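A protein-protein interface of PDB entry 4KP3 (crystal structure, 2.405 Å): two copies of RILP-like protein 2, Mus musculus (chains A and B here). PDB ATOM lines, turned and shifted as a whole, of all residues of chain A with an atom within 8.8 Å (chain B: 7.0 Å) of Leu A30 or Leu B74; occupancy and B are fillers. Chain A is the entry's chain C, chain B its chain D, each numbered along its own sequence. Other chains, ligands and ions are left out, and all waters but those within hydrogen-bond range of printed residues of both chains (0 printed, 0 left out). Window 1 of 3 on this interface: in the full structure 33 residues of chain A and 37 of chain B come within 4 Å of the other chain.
Among the printed residues, pairs that only touch across the chains: Pro A29 with Met B70 (3.96 Å), Pro A29 with Thr B73 (3.8 Å), Pro A29 with Leu B74 (3.6 Å), Leu A30 with Leu B74 (3.9 Å), Leu A30 with Glu B77 (3.9 Å), Leu A32 with Met B70 (3.6 Å), Leu A71 with Leu B71 (3.9 Å), Leu A74 with Leu B71 (3.4 Å), Leu A74 with Val B75 (3.5 Å) and Val A75 with Leu B74 (3.6 Å).
Hydrophobic or aromatic side chains of chain B that line the printed part of chain A: Met B70, Leu B71, Leu B74 and Val B75. Along chain B the printed residues that touch a printed residue of chain A span positions 70 to 77. Of the 21 printed residues of chain A, 6 touch a printed residue of chain B. Hydrophobic or aromatic side chains of chain A that line the printed part of chain B: Pro A29, Leu A30, Leu A32, Leu A71, Leu A74 and Val A75. Among the printed residues, 10 pairs touch across the chains. Among the printed residues, no Asp or Glu carboxylate lies within 4 Å of a Lys or Arg side-chain nitrogen of the other chain.
The side-chain hydroxyl of Thr B73 lies within hydrogen-bond range of the backbone carbonyl oxygen of Glu B69, at 3.1 Å.
Of the printed residues of chain B, Leu A32 touches Met B70 (3.6 Å). Of the printed residues of chain A, Leu B71 touches Leu A71 and Leu A74. Leu B74 touches three residues of chain A. The nearest residue of chain A that does not touch Leu B74 is Leu A71 (4.02 Å).
Leu A71 touches its own counterpart, Leu B71. Leu A74 touches Leu B71, but with the chains exchanged Leu A71 does not touch Leu B74 (4.02 Å). Leu A74 touches Val B75, and with the chains exchanged Val A75 touches Leu B74. 10 positions are printed for both chains.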
ATOM      1  N   ALA A  24      17.658 -12.064  15.734  1.00  0.00           N
ATOM      2  CA  ALA A  24      17.081 -12.826  14.632  1.00  0.00           C
ATOM      3  C   ALA A  24      17.288 -14.338  14.793  1.00  0.00           C
ATOM      4  O   ALA A  24      16.382 -15.123  14.520  1.00  0.00           O
ATOM      5  CB  ALA A  24      17.620 -12.331  13.289  1.00  0.00           C
ATOM      6  N   LYS A  27      14.722 -15.851  17.026  1.00  0.00           N
ATOM      7  CA  LYS A  27      13.339 -15.820  16.574  1.00  0.00           C
ATOM      8  C   LYS A  27      12.860 -17.218  16.210  1.00  0.00           C
ATOM      9  O   LYS A  27      13.645 -18.061  15.782  1.00  0.00           O
ATOM     10  CB  LYS A  27      13.179 -14.910  15.355  1.00  0.00           C
ATOM     11  CG  LYS A  27      13.001 -13.431  15.665  1.00  0.00           C
ATOM     12  CD  LYS A  27      11.955 -12.822  14.733  1.00  0.00           C
ATOM     13  CE  LYS A  27      12.169 -11.339  14.532  1.00  0.00           C
ATOM     14  NZ  LYS A  27      11.272 -10.803  13.463  1.00  0.00           N
ATOM     15  N   SER A  28      11.568 -17.459  16.391  1.00  0.00           N
ATOM     16  CA  SER A  28      10.934 -18.613  15.785  1.00  0.00           C
ATOM     17  C   SER A  28      11.027 -18.430  14.281  1.00  0.00           C
ATOM     18  O   SER A  28      10.813 -17.326  13.776  1.00  0.00           O
ATOM     19  CB  SER A  28       9.468 -18.701  16.197  1.00  0.00           C
ATOM     20  OG  SER A  28       8.792 -19.684  15.434  1.00  0.00           O
ATOM     21  N   PRO A  29      11.348 -19.509  13.556  1.00  0.00           N
ATOM     22  CA  PRO A  29      11.516 -19.431  12.098  1.00  0.00           C
ATOM     23  C   PRO A  29      10.284 -18.863  11.386  1.00  0.00           C
ATOM     24  O   PRO A  29      10.432 -18.116  10.418  1.00  0.00           O
ATOM     25  CB  PRO A  29      11.737 -20.889  11.690  1.00  0.00           C
ATOM     26  CG  PRO A  29      12.231 -21.563  12.922  1.00  0.00           C
ATOM     27  CD  PRO A  29      11.566 -20.872  14.071  1.00  0.00           C
ATOM     28  N   LEU A  30       9.093 -19.202  11.865  1.00  0.00           N
ATOM     29  CA  LEU A  30       7.861 -18.727  11.236  1.00  0.00           C
ATOM     30  C   LEU A  30       7.659 -17.220  11.394  1.00  0.00           C
ATOM     31  O   LEU A  30       6.829 -16.629  10.711  1.00  0.00           O
ATOM     32  CB  LEU A  30       6.644 -19.476  11.783  1.00  0.00           C
ATOM     33  CG  LEU A  30       6.531 -20.962  11.447  1.00  0.00           C
ATOM     34  CD1 LEU A  30       5.442 -21.606  12.279  1.00  0.00           C
ATOM     35  CD2 LEU A  30       6.249 -21.163   9.969  1.00  0.00           C
ATOM     36  N   GLN A  31       8.424 -16.597  12.284  1.00  0.00           N
ATOM     37  CA  GLN A  31       8.314 -15.159  12.502  1.00  0.00           C
ATOM     38  C   GLN A  31       9.516 -14.379  11.969  1.00  0.00           C
ATOM     39  O   GLN A  31       9.667 -13.189  12.252  1.00  0.00           O
ATOM     40  CB  GLN A  31       8.104 -14.863  13.986  1.00  0.00           C
ATOM     41  CG  GLN A  31       6.872 -15.535  14.572  1.00  0.00           C
ATOM     42  CD  GLN A  31       6.736 -15.292  16.057  1.00  0.00           C
ATOM     43  OE1 GLN A  31       7.320 -14.354  16.600  1.00  0.00           O
ATOM     44  NE2 GLN A  31       5.966 -16.144  16.729  1.00  0.00           N
ATOM     45  N   LEU A  32      10.367 -15.052  11.199  1.00  0.00           N
ATOM     46  CA  LEU A  32      11.491 -14.393  10.548  1.00  0.00           C
ATOM     47  C   LEU A  32      10.998 -13.497   9.426  1.00  0.00           C
ATOM     48  O   LEU A  32      10.067 -13.848   8.704  1.00  0.00           O
ATOM     49  CB  LEU A  32      12.468 -15.422   9.970  1.00  0.00           C
ATOM     50  CG  LEU A  32      13.451 -16.144  10.890  1.00  0.00           C
ATOM     51  CD1 LEU A  32      14.255 -17.154  10.090  1.00  0.00           C
ATOM     52  CD2 LEU A  32      14.373 -15.153  11.582  1.00  0.00           C
ATOM     53  N   THR A  33      11.626 -12.338   9.284  1.00  0.00           N
ATOM     54  CA  THR A  33      11.378 -11.472   8.141  1.00  0.00           C
ATOM     55  C   THR A  33      12.610 -11.491   7.259  1.00  0.00           C
ATOM     56  O   THR A  33      13.676 -11.950   7.677  1.00  0.00           O
ATOM     57  CB  THR A  33      11.135 -10.027   8.575  1.00  0.00           C
ATOM     58  OG1 THR A  33      12.332  -9.504   9.159  1.00  0.00           O
ATOM     59  CG2 THR A  33      10.013  -9.964   9.593  1.00  0.00           C
ATOM     60  N   ASP A  36      15.489  -9.918   8.904  1.00  0.00           N
ATOM     61  CA  ASP A  36      16.211 -10.821   9.801  1.00  0.00           C
ATOM     62  C   ASP A  36      17.258 -11.614   9.027  1.00  0.00           C
ATOM     63  O   ASP A  36      18.405 -11.736   9.460  1.00  0.00           O
ATOM     64  CB  ASP A  36      15.250 -11.794  10.482  1.00  0.00           C
ATOM     65  CG  ASP A  36      14.286 -11.104  11.423  1.00  0.00           C
ATOM     66  OD1 ASP A  36      14.712 -10.171  12.134  1.00  0.00           O
ATOM     67  OD2 ASP A  36      13.100 -11.497  11.446  1.00  0.00           O
ATOM     68  N   VAL A  37      16.850 -12.141   7.876  1.00  0.00           N
ATOM     69  CA  VAL A  37      17.742 -12.880   6.993  1.00  0.00           C
ATOM     70  C   VAL A  37      18.936 -12.021   6.577  1.00  0.00           C
ATOM     71  O   VAL A  37      20.077 -12.478   6.612  1.00  0.00           O
ATOM     72  CB  VAL A  37      16.998 -13.380   5.739  1.00  0.00           C
ATOM     73  CG1 VAL A  37      17.952 -14.106   4.804  1.00  0.00           C
ATOM     74  CG2 VAL A  37      15.836 -14.286   6.138  1.00  0.00           C
ATOM     75  N   MET A  70      18.317 -19.370   0.065  1.00  0.00           N
ATOM     76  CA  MET A  70      17.212 -20.311   0.176  1.00  0.00           C
ATOM     77  C   MET A  70      16.299 -19.939   1.337  1.00  0.00           C
ATOM     78  O   MET A  70      15.080 -19.928   1.194  1.00  0.00           O
ATOM     79  CB  MET A  70      17.733 -21.748   0.299  1.00  0.00           C
ATOM     80  CG  MET A  70      18.313 -22.260  -1.015  1.00  0.00           C
ATOM     81  SD  MET A  70      18.901 -23.963  -0.974  1.00  0.00           S
ATOM     82  CE  MET A  70      19.917 -23.897   0.486  1.00  0.00           C
ATOM     83  N   LEU A  71      16.901 -19.610   2.475  1.00  0.00           N
ATOM     84  CA  LEU A  71      16.163 -19.116   3.627  1.00  0.00           C
ATOM     85  C   LEU A  71      15.369 -17.845   3.293  1.00  0.00           C
ATOM     86  O   LEU A  71      14.230 -17.691   3.734  1.00  0.00           O
ATOM     87  CB  LEU A  71      17.121 -18.850   4.791  1.00  0.00           C
ATOM     88  CG  LEU A  71      16.475 -18.595   6.150  1.00  0.00           C
ATOM     89  CD1 LEU A  71      15.647 -19.797   6.593  1.00  0.00           C
ATOM     90  CD2 LEU A  71      17.531 -18.268   7.183  1.00  0.00           C
ATOM     91  N   GLU A  72      15.964 -16.942   2.516  1.00  0.00           N
ATOM     92  CA  GLU A  72      15.279 -15.707   2.135  1.00  0.00           C
ATOM     93  C   GLU A  72      14.034 -15.990   1.304  1.00  0.00           C
ATOM     94  O   GLU A  72      12.975 -15.405   1.537  1.00  0.00           O
ATOM     95  CB  GLU A  72      16.202 -14.753   1.357  1.00  0.00           C
ATOM     96  CG  GLU A  72      15.463 -13.534   0.784  1.00  0.00           C
ATOM     97  CD  GLU A  72      16.313 -12.672  -0.144  1.00  0.00           C
ATOM     98  OE1 GLU A  72      17.430 -13.091  -0.509  1.00  0.00           O
ATOM     99  OE2 GLU A  72      15.856 -11.568  -0.510  1.00  0.00           O
ATOM    100  N   THR A  73      14.174 -16.883   0.328  1.00  0.00           N
ATOM    101  CA  THR A  73      13.068 -17.244  -0.551  1.00  0.00           C
ATOM    102  C   THR A  73      11.921 -17.895   0.219  1.00  0.00           C
ATOM    103  O   THR A  73      10.753 -17.628  -0.050  1.00  0.00           O
ATOM    104  CB  THR A  73      13.525 -18.206  -1.659  1.00  0.00           C
ATOM    105  OG1 THR A  73      14.598 -17.610  -2.395  1.00  0.00           O
ATOM    106  CG2 THR A  73      12.378 -18.512  -2.610  1.00  0.00           C
ATOM    107  N   LEU A  74      12.265 -18.747   1.178  1.00  0.00           N
ATOM    108  CA  LEU A  74      11.261 -19.422   1.979  1.00  0.00           C
ATOM    109  C   LEU A  74      10.521 -18.447   2.878  1.00  0.00           C
ATOM    110  O   LEU A  74       9.297 -18.500   2.987  1.00  0.00           O
ATOM    111  CB  LEU A  74      11.896 -20.535   2.805  1.00  0.00           C
ATOM    112  CG  LEU A  74      12.299 -21.744   1.967  1.00  0.00           C
ATOM    113  CD1 LEU A  74      13.170 -22.636   2.780  1.00  0.00           C
ATOM    114  CD2 LEU A  74      11.068 -22.499   1.506  1.00  0.00           C
ATOM    115  N   VAL A  75      11.271 -17.561   3.522  1.00  0.00           N
ATOM    116  CA  VAL A  75      10.679 -16.524   4.352  1.00  0.00           C
ATOM    117  C   VAL A  75       9.728 -15.658   3.527  1.00  0.00           C
ATOM    118  O   VAL A  75       8.629 -15.326   3.970  1.00  0.00           O
ATOM    119  CB  VAL A  75      11.763 -15.636   5.000  1.00  0.00           C
ATOM    120  CG1 VAL A  75      11.154 -14.361   5.558  1.00  0.00           C
ATOM    121  CG2 VAL A  75      12.485 -16.402   6.094  1.00  0.00           C
ATOM    122  N   ASN A  76      10.143 -15.335   2.306  1.00  0.00           N
ATOM    123  CA  ASN A  76       9.444 -14.358   1.475  1.00  0.00           C
ATOM    124  C   ASN A  76       8.306 -14.924   0.615  1.00  0.00           C
ATOM    125  O   ASN A  76       7.350 -14.215   0.305  1.00  0.00           O
ATOM    126  CB  ASN A  76      10.463 -13.615   0.600  1.00  0.00           C
ATOM    127  CG  ASN A  76       9.852 -12.466  -0.170  1.00  0.00           C
ATOM    128  OD1 ASN A  76       9.448 -11.457   0.411  1.00  0.00           O
ATOM    129  ND2 ASN A  76       9.799 -12.602  -1.490  1.00  0.00           N
ATOM    130  N   GLU A  77       8.406 -16.195   0.230  1.00  0.00           N
ATOM    131  CA  GLU A  77       7.433 -16.793  -0.685  1.00  0.00           C
ATOM    132  C   GLU A  77       6.818 -18.089  -0.155  1.00  0.00           C
ATOM    133  O   GLU A  77       5.957 -18.680  -0.808  1.00  0.00           O
ATOM    134  CB  GLU A  77       8.076 -17.071  -2.048  1.00  0.00           C
ATOM    135  CG  GLU A  77       8.722 -15.869  -2.717  1.00  0.00           C
ATOM    136  CD  GLU A  77       9.486 -16.250  -3.973  1.00  0.00           C
ATOM    137  OE1 GLU A  77       9.220 -17.344  -4.517  1.00  0.00           O
ATOM    138  OE2 GLU A  77      10.356 -15.464  -4.411  1.00  0.00           O
ATOM    139  N   GLY A  78       7.263 -18.533   1.017  1.00  0.00           N
ATOM    140  CA  GLY A  78       6.791 -19.783   1.594  1.00  0.00           C
ATOM    141  C   GLY A  78       5.294 -19.870   1.851  1.00  0.00           C
ATOM    142  O   GLY A  78       4.724 -20.960   1.818  1.00  0.00           O
ATOM    143  N   SER A  79       4.661 -18.723   2.096  1.00  0.00           N
ATOM    144  CA  SER A  79       3.235 -18.668   2.423  1.00  0.00           C
ATOM    145  C   SER A  79       2.339 -18.671   1.192  1.00  0.00           C
ATOM    146  O   SER A  79       1.155 -18.992   1.289  1.00  0.00           O
ATOM    147  CB  SER A  79       2.918 -17.414   3.242  1.00  0.00           C
ATOM    148  OG  SER A  79       3.602 -17.413   4.479  1.00  0.00           O
ATOM    149  N   VAL A  82       0.532 -21.919   0.125  1.00  0.00           N
ATOM    150  CA  VAL A  82      -0.419 -22.189   1.198  1.00  0.00           C
ATOM    151  C   VAL A  82      -1.616 -21.245   1.107  1.00  0.00           C
ATOM    152  O   VAL A  82      -2.762 -21.683   1.200  1.00  0.00           O
ATOM    153  CB  VAL A  82       0.237 -22.054   2.586  1.00  0.00           C
ATOM    154  CG1 VAL A  82      -0.823 -22.085   3.683  1.00  0.00           C
ATOM    155  CG2 VAL A  82       1.270 -23.153   2.800  1.00  0.00           C
ATOM    156  N   MET B  68      20.470 -23.615   9.680  1.00  0.00           N
ATOM    157  CA  MET B  68      19.966 -24.828   9.044  1.00  0.00           C
ATOM    158  C   MET B  68      18.691 -25.327   9.728  1.00  0.00           C
ATOM    159  O   MET B  68      17.771 -25.805   9.062  1.00  0.00           O
ATOM    160  CB  MET B  68      21.037 -25.928   9.024  1.00  0.00           C
ATOM    161  CG  MET B  68      22.279 -25.575   8.226  1.00  0.00           C
ATOM    162  SD  MET B  68      21.899 -25.210   6.503  1.00  0.00           S
ATOM    163  CE  MET B  68      21.124 -26.732   5.978  1.00  0.00           C
ATOM    164  N   GLU B  69      18.647 -25.215  11.054  1.00  0.00           N
ATOM    165  CA  GLU B  69      17.437 -25.513  11.822  1.00  0.00           C
ATOM    166  C   GLU B  69      16.239 -24.689  11.341  1.00  0.00           C
ATOM    167  O   GLU B  69      15.135 -25.219  11.161  1.00  0.00           O
ATOM    168  CB  GLU B  69      17.674 -25.271  13.320  1.00  0.00           C
ATOM    169  CG  GLU B  69      18.459 -26.376  14.021  1.00  0.00           C
ATOM    170  CD  GLU B  69      18.814 -26.042  15.460  1.00  0.00           C
ATOM    171  OE1 GLU B  69      18.786 -24.851  15.831  1.00  0.00           O
ATOM    172  OE2 GLU B  69      19.130 -26.978  16.223  1.00  0.00           O
ATOM    173  N   MET B  70      16.463 -23.394  11.126  1.00  0.00           N
ATOM    174  CA  MET B  70      15.395 -22.506  10.675  1.00  0.00           C
ATOM    175  C   MET B  70      14.975 -22.877   9.266  1.00  0.00           C
ATOM    176  O   MET B  70      13.789 -22.853   8.936  1.00  0.00           O
ATOM    177  CB  MET B  70      15.826 -21.037  10.756  1.00  0.00           C
ATOM    178  CG  MET B  70      16.041 -20.569  12.188  1.00  0.00           C
ATOM    179  SD  MET B  70      16.517 -18.845  12.345  1.00  0.00           S
ATOM    180  CE  MET B  70      17.926 -18.791  11.260  1.00  0.00           C
ATOM    181  N   LEU B  71      15.958 -23.241   8.449  1.00  0.00           N
ATOM    182  CA  LEU B  71      15.703 -23.701   7.092  1.00  0.00           C
ATOM    183  C   LEU B  71      14.874 -24.983   7.106  1.00  0.00           C
ATOM    184  O   LEU B  71      13.896 -25.093   6.368  1.00  0.00           O
ATOM    185  CB  LEU B  71      17.022 -23.927   6.351  1.00  0.00           C
ATOM    186  CG  LEU B  71      16.911 -24.281   4.869  1.00  0.00           C
ATOM    187  CD1 LEU B  71      16.308 -23.128   4.116  1.00  0.00           C
ATOM    188  CD2 LEU B  71      18.270 -24.623   4.290  1.00  0.00           C
ATOM    189  N   GLU B  72      15.262 -25.947   7.942  1.00  0.00           N
ATOM    190  CA  GLU B  72      14.499 -27.187   8.082  1.00  0.00           C
ATOM    191  C   GLU B  72      13.041 -26.910   8.441  1.00  0.00           C
ATOM    192  O   GLU B  72      12.126 -27.416   7.784  1.00  0.00           O
ATOM    193  CB  GLU B  72      15.104 -28.125   9.139  1.00  0.00           C
ATOM    194  CG  GLU B  72      14.353 -29.469   9.224  1.00  0.00           C
ATOM    195  CD  GLU B  72      14.573 -30.227  10.529  1.00  0.00           C
ATOM    196  OE1 GLU B  72      15.358 -29.760  11.381  1.00  0.00           O
ATOM    197  OE2 GLU B  72      13.944 -31.296  10.701  1.00  0.00           O
ATOM    198  N   THR B  73      12.833 -26.099   9.477  1.00  0.00           N
ATOM    199  CA  THR B  73      11.483 -25.778   9.939  1.00  0.00           C
ATOM    200  C   THR B  73      10.606 -25.185   8.833  1.00  0.00           C
ATOM    201  O   THR B  73       9.508 -25.683   8.578  1.00  0.00           O
ATOM    202  CB  THR B  73      11.501 -24.830  11.152  1.00  0.00           C
ATOM    203  OG1 THR B  73      12.224 -25.443  12.229  1.00  0.00           O
ATOM    204  CG2 THR B  73      10.083 -24.521  11.610  1.00  0.00           C
ATOM    205  N   LEU B  74      11.095 -24.139   8.170  1.00  0.00           N
ATOM    206  CA  LEU B  74      10.330 -23.485   7.106  1.00  0.00           C
ATOM    207  C   LEU B  74      10.034 -24.423   5.939  1.00  0.00           C
ATOM    208  O   LEU B  74       8.946 -24.376   5.364  1.00  0.00           O
ATOM    209  CB  LEU B  74      11.041 -22.223   6.607  1.00  0.00           C
ATOM    210  CG  LEU B  74      11.051 -21.046   7.582  1.00  0.00           C
ATOM    211  CD1 LEU B  74      11.639 -19.812   6.925  1.00  0.00           C
ATOM    212  CD2 LEU B  74       9.651 -20.764   8.090  1.00  0.00           C
ATOM    213  N   VAL B  75      10.998 -25.269   5.589  1.00  0.00           N
ATOM    214  CA  VAL B  75      10.770 -26.279   4.561  1.00  0.00           C
ATOM    215  C   VAL B  75       9.703 -27.273   5.026  1.00  0.00           C
ATOM    216  O   VAL B  75       8.760 -27.573   4.292  1.00  0.00           O
ATOM    217  CB  VAL B  75      12.078 -27.019   4.178  1.00  0.00           C
ATOM    218  CG1 VAL B  75      11.780 -28.273   3.348  1.00  0.00           C
ATOM    219  CG2 VAL B  75      13.015 -26.089   3.420  1.00  0.00           C
ATOM    220  N   ASN B  76       9.843 -27.756   6.259  1.00  0.00           N
ATOM    221  CA  ASN B  76       8.908 -28.733   6.823  1.00  0.00           C
ATOM    222  C   ASN B  76       7.478 -28.212   6.950  1.00  0.00           C
ATOM    223  O   ASN B  76       6.536 -28.852   6.481  1.00  0.00           O
ATOM    224  CB  ASN B  76       9.398 -29.218   8.186  1.00  0.00           C
ATOM    225  CG  ASN B  76       8.554 -30.348   8.739  1.00  0.00           C
ATOM    226  OD1 ASN B  76       8.222 -31.299   8.031  1.00  0.00           O
ATOM    227  ND2 ASN B  76       8.194 -30.244  10.010  1.00  0.00           N
ATOM    228  N   GLU B  77       7.327 -27.056   7.595  1.00  0.00           N
ATOM    229  CA  GLU B  77       6.036 -26.390   7.741  1.00  0.00           C
ATOM    230  C   GLU B  77       5.320 -26.215   6.410  1.00  0.00           C
ATOM    231  O   GLU B  77       4.152 -26.576   6.271  1.00  0.00           O
ATOM    232  CB  GLU B  77       6.221 -25.013   8.384  1.00  0.00           C
ATOM    233  CG  GLU B  77       6.674 -25.066   9.826  1.00  0.00           C
ATOM    234  CD  GLU B  77       5.726 -25.866  10.693  1.00  0.00           C
ATOM    235  OE1 GLU B  77       4.502 -25.648  10.586  1.00  0.00           O
ATOM    236  OE2 GLU B  77       6.206 -26.719  11.471  1.00  0.00           O
ATOM    237  N   GLY B  78       6.032 -25.651   5.438  1.00  0.00           N
ATOM    238  CA  GLY B  78       5.472 -25.395   4.124  1.00  0.00           C
ATOM    239  C   GLY B  78       4.969 -26.647   3.430  1.00  0.00           C
ATOM    240  O   GLY B  78       3.867 -26.662   2.888  1.00  0.00           O
ATOM    241  N   SER B  79       5.780 -27.698   3.456  1.00  0.00           N
ATOM    242  CA  SER B  79       5.412 -28.966   2.838  1.00  0.00           C
ATOM    243  C   SER B  79       4.192 -29.605   3.510  1.00  0.00           C
ATOM    244  O   SER B  79       3.254 -30.028   2.832  1.00  0.00           O
ATOM    245  CB  SER B  79       6.604 -29.928   2.849  1.00  0.00           C
ATOM    246  OG  SER B  79       6.248 -31.198   2.333  1.00  0.00           O
